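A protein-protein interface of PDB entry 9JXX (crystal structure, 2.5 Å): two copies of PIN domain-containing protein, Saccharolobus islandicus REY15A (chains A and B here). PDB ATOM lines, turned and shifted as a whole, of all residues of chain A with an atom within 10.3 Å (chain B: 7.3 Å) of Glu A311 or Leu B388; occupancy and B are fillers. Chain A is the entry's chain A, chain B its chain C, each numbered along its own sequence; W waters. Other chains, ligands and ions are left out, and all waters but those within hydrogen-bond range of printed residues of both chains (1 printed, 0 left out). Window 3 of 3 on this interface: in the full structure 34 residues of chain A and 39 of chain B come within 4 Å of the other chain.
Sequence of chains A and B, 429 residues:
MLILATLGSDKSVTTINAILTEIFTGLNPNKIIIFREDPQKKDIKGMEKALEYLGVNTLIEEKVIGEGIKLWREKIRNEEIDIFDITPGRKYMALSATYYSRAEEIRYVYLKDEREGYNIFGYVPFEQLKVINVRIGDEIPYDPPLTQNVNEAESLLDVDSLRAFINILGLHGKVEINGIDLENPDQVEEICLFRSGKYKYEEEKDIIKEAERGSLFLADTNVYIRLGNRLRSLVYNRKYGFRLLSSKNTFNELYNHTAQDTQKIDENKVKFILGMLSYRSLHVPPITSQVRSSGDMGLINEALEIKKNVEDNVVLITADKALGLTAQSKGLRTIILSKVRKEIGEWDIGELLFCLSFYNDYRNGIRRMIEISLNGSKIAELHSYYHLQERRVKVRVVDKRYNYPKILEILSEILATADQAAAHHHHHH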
ATOM      1  N   ARG A 213      16.802  17.631   8.617  1.00  0.00           N
ATOM      2  CA  ARG A 213      17.317  18.992   8.568  1.00  0.00           C
ATOM      3  C   ARG A 213      17.961  19.336   7.230  1.00  0.00           C
ATOM      4  O   ARG A 213      18.442  20.461   7.064  1.00  0.00           O
ATOM      5  CB  ARG A 213      18.319  19.209   9.706  1.00  0.00           C
ATOM      6  CG  ARG A 213      17.744  18.884  11.075  1.00  0.00           C
ATOM      7  CD  ARG A 213      18.804  18.883  12.163  1.00  0.00           C
ATOM      8  NE  ARG A 213      18.205  19.002  13.488  1.00  0.00           N
ATOM      9  CZ  ARG A 213      18.869  19.340  14.584  1.00  0.00           C
ATOM     10  NH1 ARG A 213      20.167  19.592  14.557  1.00  0.00           N
ATOM     11  NH2 ARG A 213      18.213  19.427  15.738  1.00  0.00           N
ATOM     12  N   GLY A 214      17.985  18.401   6.281  1.00  0.00           N
ATOM     13  CA  GLY A 214      18.450  18.704   4.942  1.00  0.00           C
ATOM     14  C   GLY A 214      19.945  18.672   4.738  1.00  0.00           C
ATOM     15  O   GLY A 214      20.442  19.305   3.802  1.00  0.00           O
ATOM     16  N   SER A 215      20.684  17.958   5.582  1.00  0.00           N
ATOM     17  CA  SER A 215      22.123  17.867   5.402  1.00  0.00           C
ATOM     18  C   SER A 215      22.465  16.930   4.245  1.00  0.00           C
ATOM     19  O   SER A 215      21.682  16.057   3.862  1.00  0.00           O
ATOM     20  CB  SER A 215      22.793  17.374   6.686  1.00  0.00           C
ATOM     21  OG  SER A 215      22.159  17.910   7.835  1.00  0.00           O
ATOM     22  N   LEU A 216      23.651  17.133   3.678  1.00  0.00           N
ATOM     23  CA  LEU A 216      24.240  16.183   2.745  1.00  0.00           C
ATOM     24  C   LEU A 216      25.157  15.228   3.498  1.00  0.00           C
ATOM     25  O   LEU A 216      25.755  15.587   4.517  1.00  0.00           O
ATOM     26  CB  LEU A 216      25.033  16.900   1.652  1.00  0.00           C
ATOM     27  CG  LEU A 216      24.275  17.587   0.516  1.00  0.00           C
ATOM     28  CD1 LEU A 216      25.266  18.265  -0.416  1.00  0.00           C
ATOM     29  CD2 LEU A 216      23.401  16.598  -0.246  1.00  0.00           C
ATOM     30  N   TYR A 240      13.589  17.323   0.904  1.00  0.00           N
ATOM     31  CA  TYR A 240      14.765  17.516   0.064  1.00  0.00           C
ATOM     32  C   TYR A 240      15.179  16.277  -0.721  1.00  0.00           C
ATOM     33  O   TYR A 240      16.031  16.390  -1.609  1.00  0.00           O
ATOM     34  CB  TYR A 240      15.961  17.999   0.905  1.00  0.00           C
ATOM     35  CG  TYR A 240      15.614  18.996   1.995  1.00  0.00           C
ATOM     36  CD1 TYR A 240      15.727  20.363   1.778  1.00  0.00           C
ATOM     37  CD2 TYR A 240      15.206  18.569   3.250  1.00  0.00           C
ATOM     38  CE1 TYR A 240      15.418  21.274   2.774  1.00  0.00           C
ATOM     39  CE2 TYR A 240      14.892  19.468   4.250  1.00  0.00           C
ATOM     40  CZ  TYR A 240      15.002  20.819   4.009  1.00  0.00           C
ATOM     41  OH  TYR A 240      14.695  21.717   5.006  1.00  0.00           O
ATOM     42  N   ARG A 243      19.641  12.447   0.245  1.00  0.00           N
ATOM     43  CA  ARG A 243      20.657  13.328   0.806  1.00  0.00           C
ATOM     44  C   ARG A 243      22.062  12.740   0.790  1.00  0.00           C
ATOM     45  O   ARG A 243      22.995  13.401   1.254  1.00  0.00           O
ATOM     46  CB  ARG A 243      20.284  13.704   2.243  1.00  0.00           C
ATOM     47  CG  ARG A 243      18.935  14.385   2.376  1.00  0.00           C
ATOM     48  CD  ARG A 243      18.797  15.522   1.379  1.00  0.00           C
ATOM     49  NE  ARG A 243      19.565  16.695   1.777  1.00  0.00           N
ATOM     50  CZ  ARG A 243      19.956  17.650   0.944  1.00  0.00           C
ATOM     51  NH1 ARG A 243      19.674  17.599  -0.348  1.00  0.00           N
ATOM     52  NH2 ARG A 243      20.643  18.685   1.420  1.00  0.00           N
ATOM     53  N   LEU A 245      25.421  11.862  -0.868  1.00  0.00           N
ATOM     54  CA  LEU A 245      26.319  12.069  -1.993  1.00  0.00           C
ATOM     55  C   LEU A 245      27.109  10.799  -2.280  1.00  0.00           C
ATOM     56  O   LEU A 245      27.378   9.992  -1.386  1.00  0.00           O
ATOM     57  CB  LEU A 245      27.289  13.217  -1.714  1.00  0.00           C
ATOM     58  CG  LEU A 245      26.703  14.625  -1.670  1.00  0.00           C
ATOM     59  CD1 LEU A 245      27.742  15.618  -1.166  1.00  0.00           C
ATOM     60  CD2 LEU A 245      26.180  15.024  -3.041  1.00  0.00           C
ATOM     61  N   GLU A 305      36.256  19.566   1.029  1.00  0.00           N
ATOM     62  CA  GLU A 305      36.175  20.305  -0.229  1.00  0.00           C
ATOM     63  C   GLU A 305      34.726  20.540  -0.637  1.00  0.00           C
ATOM     64  O   GLU A 305      34.372  21.634  -1.094  1.00  0.00           O
ATOM     65  CB  GLU A 305      36.927  19.557  -1.328  1.00  0.00           C
ATOM     66  CG  GLU A 305      38.338  20.068  -1.583  1.00  0.00           C
ATOM     67  CD  GLU A 305      38.421  21.583  -1.602  1.00  0.00           C
ATOM     68  OE1 GLU A 305      38.857  22.171  -0.590  1.00  0.00           O
ATOM     69  OE2 GLU A 305      38.051  22.187  -2.632  1.00  0.00           O
ATOM     70  N   ILE A 306      33.874  19.525  -0.482  1.00  0.00           N
ATOM     71  CA  ILE A 306      32.453  19.697  -0.768  1.00  0.00           C
ATOM     72  C   ILE A 306      31.847  20.723   0.181  1.00  0.00           C
ATOM     73  O   ILE A 306      31.120  21.631  -0.240  1.00  0.00           O
ATOM     74  CB  ILE A 306      31.723  18.344  -0.681  1.00  0.00           C
ATOM     75  CG1 ILE A 306      31.886  17.568  -1.990  1.00  0.00           C
ATOM     76  CG2 ILE A 306      30.250  18.546  -0.352  1.00  0.00           C
ATOM     77  CD1 ILE A 306      32.085  16.083  -1.792  1.00  0.00           C
ATOM     78  N   LYS A 307      32.162  20.603   1.474  1.00  0.00           N
ATOM     79  CA  LYS A 307      31.627  21.519   2.477  1.00  0.00           C
ATOM     80  C   LYS A 307      31.957  22.969   2.147  1.00  0.00           C
ATOM     81  O   LYS A 307      31.113  23.859   2.310  1.00  0.00           O
ATOM     82  CB  LYS A 307      32.180  21.149   3.855  1.00  0.00           C
ATOM     83  CG  LYS A 307      31.715  22.040   4.989  1.00  0.00           C
ATOM     84  CD  LYS A 307      32.480  21.728   6.263  1.00  0.00           C
ATOM     85  CE  LYS A 307      31.826  22.361   7.476  1.00  0.00           C
ATOM     86  NZ  LYS A 307      32.323  21.746   8.738  1.00  0.00           N
ATOM     87  N   LYS A 308      33.179  23.224   1.677  1.00  0.00           N
ATOM     88  CA  LYS A 308      33.609  24.589   1.402  1.00  0.00           C
ATOM     89  C   LYS A 308      32.806  25.227   0.273  1.00  0.00           C
ATOM     90  O   LYS A 308      32.649  26.453   0.241  1.00  0.00           O
ATOM     91  CB  LYS A 308      35.104  24.592   1.070  1.00  0.00           C
ATOM     92  CG  LYS A 308      35.662  25.918   0.586  1.00  0.00           C
ATOM     93  CD  LYS A 308      37.153  25.812   0.313  1.00  0.00           C
ATOM     94  CE  LYS A 308      37.630  26.932  -0.594  1.00  0.00           C
ATOM     95  NZ  LYS A 308      39.105  27.121  -0.515  1.00  0.00           N
ATOM     96  N   ASN A 309      32.274  24.421  -0.645  1.00  0.00           N
ATOM     97  CA  ASN A 309      31.745  24.940  -1.899  1.00  0.00           C
ATOM     98  C   ASN A 309      30.246  24.745  -2.093  1.00  0.00           C
ATOM     99  O   ASN A 309      29.735  25.092  -3.165  1.00  0.00           O
ATOM    100  CB  ASN A 309      32.490  24.303  -3.080  1.00  0.00           C
ATOM    101  CG  ASN A 309      33.963  24.669  -3.106  1.00  0.00           C
ATOM    102  OD1 ASN A 309      34.330  25.830  -2.922  1.00  0.00           O
ATOM    103  ND2 ASN A 309      34.814  23.674  -3.326  1.00  0.00           N
ATOM    104  N   VAL A 310      29.519  24.218  -1.109  1.00  0.00           N
ATOM    105  CA  VAL A 310      28.092  23.979  -1.280  1.00  0.00           C
ATOM    106  C   VAL A 310      27.316  24.709  -0.193  1.00  0.00           C
ATOM    107  O   VAL A 310      27.830  25.014   0.887  1.00  0.00           O
ATOM    108  CB  VAL A 310      27.737  22.477  -1.272  1.00  0.00           C
ATOM    109  CG1 VAL A 310      28.467  21.749  -2.392  1.00  0.00           C
ATOM    110  CG2 VAL A 310      28.035  21.860   0.087  1.00  0.00           C
ATOM    111  N   GLU A 311      26.049  24.992  -0.505  1.00  0.00           N
ATOM    112  CA  GLU A 311      25.155  25.629   0.455  1.00  0.00           C
ATOM    113  C   GLU A 311      24.731  24.664   1.555  1.00  0.00           C
ATOM    114  O   GLU A 311      24.430  25.092   2.674  1.00  0.00           O
ATOM    115  CB  GLU A 311      23.924  26.171  -0.274  1.00  0.00           C
ATOM    116  CG  GLU A 311      23.475  27.558   0.153  1.00  0.00           C
ATOM    117  CD  GLU A 311      22.035  27.841  -0.239  1.00  0.00           C
ATOM    118  OE1 GLU A 311      21.404  26.960  -0.861  1.00  0.00           O
ATOM    119  OE2 GLU A 311      21.536  28.944   0.069  1.00  0.00           O
ATOM    120  N   ASP A 312      24.703  23.369   1.255  1.00  0.00           N
ATOM    121  CA  ASP A 312      24.167  22.388   2.186  1.00  0.00           C
ATOM    122  C   ASP A 312      25.124  22.140   3.346  1.00  0.00           C
ATOM    123  O   ASP A 312      26.341  22.316   3.233  1.00  0.00           O
ATOM    124  CB  ASP A 312      23.890  21.069   1.465  1.00  0.00           C
ATOM    125  CG  ASP A 312      23.316  21.268   0.076  1.00  0.00           C
ATOM    126  OD1 ASP A 312      24.023  21.823  -0.793  1.00  0.00           O
ATOM    127  OD2 ASP A 312      22.160  20.855  -0.153  1.00  0.00           O
ATOM    128  N   ASN A 313      24.555  21.730   4.476  1.00  0.00           N
ATOM    129  CA  ASN A 313      25.357  21.220   5.578  1.00  0.00           C
ATOM    130  C   ASN A 313      25.873  19.830   5.229  1.00  0.00           C
ATOM    131  O   ASN A 313      25.115  18.976   4.760  1.00  0.00           O
ATOM    132  CB  ASN A 313      24.531  21.170   6.862  1.00  0.00           C
ATOM    133  CG  ASN A 313      24.360  22.532   7.498  1.00  0.00           C
ATOM    134  OD1 ASN A 313      23.554  23.345   7.044  1.00  0.00           O
ATOM    135  ND2 ASN A 313      25.117  22.789   8.558  1.00  0.00           N
ATOM    136  N   VAL A 314      27.162  19.599   5.461  1.00  0.00           N
ATOM    137  CA  VAL A 314      27.814  18.339   5.120  1.00  0.00           C
ATOM    138  C   VAL A 314      28.074  17.564   6.404  1.00  0.00           C
ATOM    139  O   VAL A 314      28.656  18.101   7.355  1.00  0.00           O
ATOM    140  CB  VAL A 314      29.117  18.575   4.337  1.00  0.00           C
ATOM    141  CG1 VAL A 314      29.825  17.255   4.065  1.00  0.00           C
ATOM    142  CG2 VAL A 314      28.816  19.301   3.038  1.00  0.00           C
ATOM    143  N   VAL A 315      27.637  16.306   6.428  1.00  0.00           N
ATOM    144  CA  VAL A 315      27.799  15.419   7.573  1.00  0.00           C
ATOM    145  C   VAL A 315      28.472  14.140   7.098  1.00  0.00           C
ATOM    146  O   VAL A 315      28.114  13.592   6.050  1.00  0.00           O
ATOM    147  CB  VAL A 315      26.445  15.103   8.247  1.00  0.00           C
ATOM    148  CG1 VAL A 315      26.635  14.139   9.413  1.00  0.00           C
ATOM    149  CG2 VAL A 315      25.768  16.384   8.711  1.00  0.00           C
ATOM    150  N   ILE B 273      23.749  33.353 -13.597  1.00  0.00           N
ATOM    151  CA  ILE B 273      23.505  33.041 -12.192  1.00  0.00           C
ATOM    152  C   ILE B 273      22.326  32.084 -12.058  1.00  0.00           C
ATOM    153  O   ILE B 273      22.340  31.173 -11.221  1.00  0.00           O
ATOM    154  CB  ILE B 273      23.297  34.343 -11.392  1.00  0.00           C
ATOM    155  CG1 ILE B 273      24.653  34.931 -10.996  1.00  0.00           C
ATOM    156  CG2 ILE B 273      22.437  34.110 -10.158  1.00  0.00           C
ATOM    157  CD1 ILE B 273      24.596  36.381 -10.610  1.00  0.00           C
ATOM    158  N   LEU B 277      22.806  28.475 -10.213  1.00  0.00           N
ATOM    159  CA  LEU B 277      21.976  27.998  -9.111  1.00  0.00           C
ATOM    160  C   LEU B 277      21.259  26.704  -9.477  1.00  0.00           C
ATOM    161  O   LEU B 277      21.158  25.790  -8.651  1.00  0.00           O
ATOM    162  CB  LEU B 277      20.974  29.078  -8.704  1.00  0.00           C
ATOM    163  CG  LEU B 277      21.599  30.343  -8.113  1.00  0.00           C
ATOM    164  CD1 LEU B 277      20.524  31.312  -7.643  1.00  0.00           C
ATOM    165  CD2 LEU B 277      22.551  29.994  -6.977  1.00  0.00           C
ATOM    166  N   ARG B 280      23.796  23.956  -9.285  1.00  0.00           N
ATOM    167  CA  ARG B 280      24.075  23.582  -7.902  1.00  0.00           C
ATOM    168  C   ARG B 280      22.907  22.835  -7.275  1.00  0.00           C
ATOM    169  O   ARG B 280      23.115  21.975  -6.412  1.00  0.00           O
ATOM    170  CB  ARG B 280      24.422  24.824  -7.084  1.00  0.00           C
ATOM    171  CG  ARG B 280      25.791  25.391  -7.404  1.00  0.00           C
ATOM    172  CD  ARG B 280      26.049  26.701  -6.682  1.00  0.00           C
ATOM    173  NE  ARG B 280      27.438  27.113  -6.834  1.00  0.00           N
ATOM    174  CZ  ARG B 280      28.438  26.656  -6.094  1.00  0.00           C
ATOM    175  NH1 ARG B 280      28.231  25.797  -5.109  1.00  0.00           N
ATOM    176  NH2 ARG B 280      29.677  27.064  -6.352  1.00  0.00           N
ATOM    177  N   SER B 281      21.676  23.143  -7.690  1.00  0.00           N
ATOM    178  CA  SER B 281      20.519  22.423  -7.173  1.00  0.00           C
ATOM    179  C   SER B 281      20.520  20.956  -7.581  1.00  0.00           C
ATOM    180  O   SER B 281      19.858  20.144  -6.926  1.00  0.00           O
ATOM    181  CB  SER B 281      19.228  23.087  -7.651  1.00  0.00           C
ATOM    182  OG  SER B 281      18.812  22.539  -8.890  1.00  0.00           O
ATOM    183  N   PRO B 285      29.369  20.691  -7.148  1.00  0.00           N
ATOM    184  CA  PRO B 285      30.363  21.080  -8.151  1.00  0.00           C
ATOM    185  C   PRO B 285      31.402  19.990  -8.335  1.00  0.00           C
ATOM    186  O   PRO B 285      32.192  19.710  -7.420  1.00  0.00           O
ATOM    187  CB  PRO B 285      30.982  22.351  -7.551  1.00  0.00           C
ATOM    188  CG  PRO B 285      29.863  22.945  -6.766  1.00  0.00           C
ATOM    189  CD  PRO B 285      29.144  21.762  -6.159  1.00  0.00           C
ATOM    190  N   PHE B 358      13.295  37.295  -8.684  1.00  0.00           N
ATOM    191  CA  PHE B 358      14.752  37.290  -8.616  1.00  0.00           C
ATOM    192  C   PHE B 358      15.356  38.216  -9.664  1.00  0.00           C
ATOM    193  O   PHE B 358      16.301  38.961  -9.377  1.00  0.00           O
ATOM    194  CB  PHE B 358      15.279  35.867  -8.797  1.00  0.00           C
ATOM    195  CG  PHE B 358      16.762  35.735  -8.588  1.00  0.00           C
ATOM    196  CD1 PHE B 358      17.278  35.521  -7.320  1.00  0.00           C
ATOM    197  CD2 PHE B 358      17.638  35.825  -9.657  1.00  0.00           C
ATOM    198  CE1 PHE B 358      18.642  35.399  -7.123  1.00  0.00           C
ATOM    199  CE2 PHE B 358      19.003  35.705  -9.467  1.00  0.00           C
ATOM    200  CZ  PHE B 358      19.505  35.491  -8.198  1.00  0.00           C
ATOM    201  N   TYR B 362      17.476  42.203  -8.726  1.00  0.00           N
ATOM    202  CA  TYR B 362      18.917  42.322  -8.892  1.00  0.00           C
ATOM    203  C   TYR B 362      19.348  42.879 -10.240  1.00  0.00           C
ATOM    204  O   TYR B 362      20.542  43.141 -10.417  1.00  0.00           O
ATOM    205  CB  TYR B 362      19.591  40.958  -8.674  1.00  0.00           C
ATOM    206  CG  TYR B 362      19.481  40.476  -7.247  1.00  0.00           C
ATOM    207  CD1 TYR B 362      20.314  40.980  -6.259  1.00  0.00           C
ATOM    208  CD2 TYR B 362      18.527  39.534  -6.885  1.00  0.00           C
ATOM    209  CE1 TYR B 362      20.210  40.551  -4.949  1.00  0.00           C
ATOM    210  CE2 TYR B 362      18.415  39.099  -5.579  1.00  0.00           C
ATOM    211  CZ  TYR B 362      19.259  39.609  -4.614  1.00  0.00           C
ATOM    212  OH  TYR B 362      19.146  39.173  -3.315  1.00  0.00           O
ATOM    213  N   TYR B 385      13.750  36.238  -1.675  1.00  0.00           N
ATOM    214  CA  TYR B 385      14.127  35.823  -0.332  1.00  0.00           C
ATOM    215  C   TYR B 385      15.528  35.230  -0.362  1.00  0.00           C
ATOM    216  O   TYR B 385      15.883  34.500  -1.292  1.00  0.00           O
ATOM    217  CB  TYR B 385      13.125  34.810   0.226  1.00  0.00           C
ATOM    218  CG  TYR B 385      13.229  34.591   1.717  1.00  0.00           C
ATOM    219  CD1 TYR B 385      13.116  35.654   2.605  1.00  0.00           C
ATOM    220  CD2 TYR B 385      13.422  33.320   2.238  1.00  0.00           C
ATOM    221  CE1 TYR B 385      13.204  35.457   3.970  1.00  0.00           C
ATOM    222  CE2 TYR B 385      13.510  33.112   3.600  1.00  0.00           C
ATOM    223  CZ  TYR B 385      13.400  34.182   4.461  1.00  0.00           C
ATOM    224  OH  TYR B 385      13.489  33.974   5.817  1.00  0.00           O
ATOM    225  N   TYR B 386      16.313  35.542   0.671  1.00  0.00           N
ATOM    226  CA  TYR B 386      17.739  35.224   0.656  1.00  0.00           C
ATOM    227  C   TYR B 386      17.989  33.721   0.599  1.00  0.00           C
ATOM    228  O   TYR B 386      18.935  33.268  -0.056  1.00  0.00           O
ATOM    229  CB  TYR B 386      18.419  35.822   1.889  1.00  0.00           C
ATOM    230  CG  TYR B 386      18.203  35.005   3.142  1.00  0.00           C
ATOM    231  CD1 TYR B 386      17.002  35.070   3.835  1.00  0.00           C
ATOM    232  CD2 TYR B 386      19.190  34.151   3.618  1.00  0.00           C
ATOM    233  CE1 TYR B 386      16.793  34.319   4.973  1.00  0.00           C
ATOM    234  CE2 TYR B 386      18.989  33.395   4.756  1.00  0.00           C
ATOM    235  CZ  TYR B 386      17.789  33.484   5.429  1.00  0.00           C
ATOM    236  OH  TYR B 386      17.581  32.737   6.564  1.00  0.00           O
ATOM    237  N   HIS B 387      17.164  32.933   1.285  1.00  0.00           N
ATOM    238  CA  HIS B 387      17.463  31.522   1.508  1.00  0.00           C
ATOM    239  C   HIS B 387      17.110  30.724   0.259  1.00  0.00           C
ATOM    240  O   HIS B 387      15.931  30.537  -0.057  1.00  0.00           O
ATOM    241  CB  HIS B 387      16.707  31.007   2.728  1.00  0.00           C
ATOM    242  CG  HIS B 387      17.341  29.811   3.365  1.00  0.00           C
ATOM    243  ND1 HIS B 387      17.706  28.694   2.648  1.00  0.00           N
ATOM    244  CD2 HIS B 387      17.681  29.561   4.652  1.00  0.00           C
ATOM    245  CE1 HIS B 387      18.241  27.803   3.465  1.00  0.00           C
ATOM    246  NE2 HIS B 387      18.237  28.305   4.687  1.00  0.00           N
ATOM    247  N   LEU B 388      18.137  30.239  -0.442  1.00  0.00           N
ATOM    248  CA  LEU B 388      17.959  29.533  -1.705  1.00  0.00           C
ATOM    249  C   LEU B 388      17.670  28.046  -1.535  1.00  0.00           C
ATOM    250  O   LEU B 388      17.316  27.389  -2.520  1.00  0.00           O
ATOM    251  CB  LEU B 388      19.204  29.707  -2.576  1.00  0.00           C
ATOM    252  CG  LEU B 388      19.634  31.148  -2.857  1.00  0.00           C
ATOM    253  CD1 LEU B 388      20.869  31.170  -3.742  1.00  0.00           C
ATOM    254  CD2 LEU B 388      18.496  31.932  -3.493  1.00  0.00           C
ATOM    255  N   GLN B 389      17.817  27.497  -0.329  1.00  0.00           N
ATOM    256  CA  GLN B 389      17.597  26.070  -0.126  1.00  0.00           C
ATOM    257  C   GLN B 389      16.159  25.774   0.296  1.00  0.00           C
ATOM    258  O   GLN B 389      15.524  24.870  -0.255  1.00  0.00           O
ATOM    259  CB  GLN B 389      18.597  25.528   0.901  1.00  0.00           C
ATOM    260  CG  GLN B 389      18.125  24.302   1.663  1.00  0.00           C
ATOM    261  CD  GLN B 389      18.947  24.045   2.913  1.00  0.00           C
ATOM    262  OE1 GLN B 389      18.446  23.506   3.899  1.00  0.00           O
ATOM    263  NE2 GLN B 389      20.218  24.429   2.876  1.00  0.00           N
ATOM    264  N   GLU B 390      15.633  26.518   1.267  1.00  0.00           N
ATOM    265  CA  GLU B 390      14.200  26.510   1.566  1.00  0.00           C
ATOM    266  C   GLU B 390      13.612  27.679   0.784  1.00  0.00           C
ATOM    267  O   GLU B 390      13.469  28.790   1.296  1.00  0.00           O
ATOM    268  CB  GLU B 390      13.930  26.613   3.064  1.00  0.00           C
ATOM    269  CG  GLU B 390      14.909  27.493   3.820  1.00  0.00           C
ATOM    270  CD  GLU B 390      14.539  27.669   5.281  1.00  0.00           C
ATOM    271  OE1 GLU B 390      13.625  28.470   5.572  1.00  0.00           O
ATOM    272  OE2 GLU B 390      15.167  27.012   6.137  1.00  0.00           O
ATOM    273  N   ARG B 391      13.271  27.417  -0.475  1.00  0.00           N
ATOM    274  CA  ARG B 391      12.985  28.486  -1.422  1.00  0.00           C
ATOM    275  C   ARG B 391      11.637  29.125  -1.122  1.00  0.00           C
ATOM    276  O   ARG B 391      10.594  28.467  -1.197  1.00  0.00           O
ATOM    277  CB  ARG B 391      13.021  27.944  -2.847  1.00  0.00           C
ATOM    278  CG  ARG B 391      14.397  28.015  -3.479  1.00  0.00           C
ATOM    279  CD  ARG B 391      14.305  28.349  -4.948  1.00  0.00           C
ATOM    280  NE  ARG B 391      13.128  27.738  -5.552  1.00  0.00           N
ATOM    281  CZ  ARG B 391      12.782  27.877  -6.823  1.00  0.00           C
ATOM    282  NH1 ARG B 391      13.498  28.611  -7.659  1.00  0.00           N
ATOM    283  NH2 ARG B 391      11.691  27.261  -7.268  1.00  0.00           N
ATOM    284  N   ARG B 392      11.662  30.413  -0.790  1.00  0.00           N
ATOM    285  CA  ARG B 392      10.461  31.176  -0.500  1.00  0.00           C
ATOM    286  C   ARG B 392      10.478  32.473  -1.293  1.00  0.00           C
ATOM    287  O   ARG B 392      11.515  32.908  -1.802  1.00  0.00           O
ATOM    288  CB  ARG B 392      10.335  31.497   0.997  1.00  0.00           C
ATOM    289  CG  ARG B 392      10.528  30.310   1.921  1.00  0.00           C
ATOM    290  CD  ARG B 392       9.244  29.516   2.070  1.00  0.00           C
ATOM    291  NE  ARG B 392       9.127  28.921   3.394  1.00  0.00           N
ATOM    292  CZ  ARG B 392       9.681  27.768   3.748  1.00  0.00           C
ATOM    293  NH1 ARG B 392      10.408  27.062   2.898  1.00  0.00           N
ATOM    294  NH2 ARG B 392       9.502  27.314   4.984  1.00  0.00           N
HETATM  295  O   HOH W   1      22.840  25.057   4.542  1.00  0.00           O
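O of Asn A309 is in hydrogen-bond range of NH1 of Arg B280 (2.6 Å).
The backbone NH (N) of Gln B389 sits at hydrogen-bond distance from a ring nitrogen (ND1) of His B387 (3.2 Å). The side-chain amide nitrogen (ND2) of Asn A309 sits at hydrogen-bond distance from the backbone carbonyl oxygen (O) of Glu A305 (3.1 Å).
Among the printed residues, pairs that only touch across the chains: Tyr A240 with Gln B389 (3.9 Å), Val A310 with Pro B285 (3.8 Å), Glu A311 with Leu B388 (3.6 Å) and Glu A311 with Gln B389 (3.6 Å).
Leu B388 touches one residue of chain A. Of the printed residues of chain B, Asn A309 touches Arg B280 (2.6 Å). Of the printed residues of chain A, Pro B285 touches Val A310 (3.8 Å). Printed residues of chain A within 4 Å of Arg B280: Asn A309. The nearest residue of chain B that does not touch Glu A311 is His B387 (4.6 Å).
Hydrophobic or aromatic side chains of chain A within 4 Å of the printed part of chain B: Tyr A240 and Val A310. Hydrophobic or aromatic side chains of chain B within 4 Å of the printed part of chain A: Pro B285 and Leu B388. Among the printed residues, 5 pairs touch across the chains. Among the printed residues, no Asp or Glu carboxylate lies within 4 Å of a Lys or Arg side-chain nitrogen of the other chain.
No position is printed for both chains.
Water W1 lies within hydrogen-bond range of O of Glu A311, OD1 of Asn A313 and NE2 of Gln B389.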
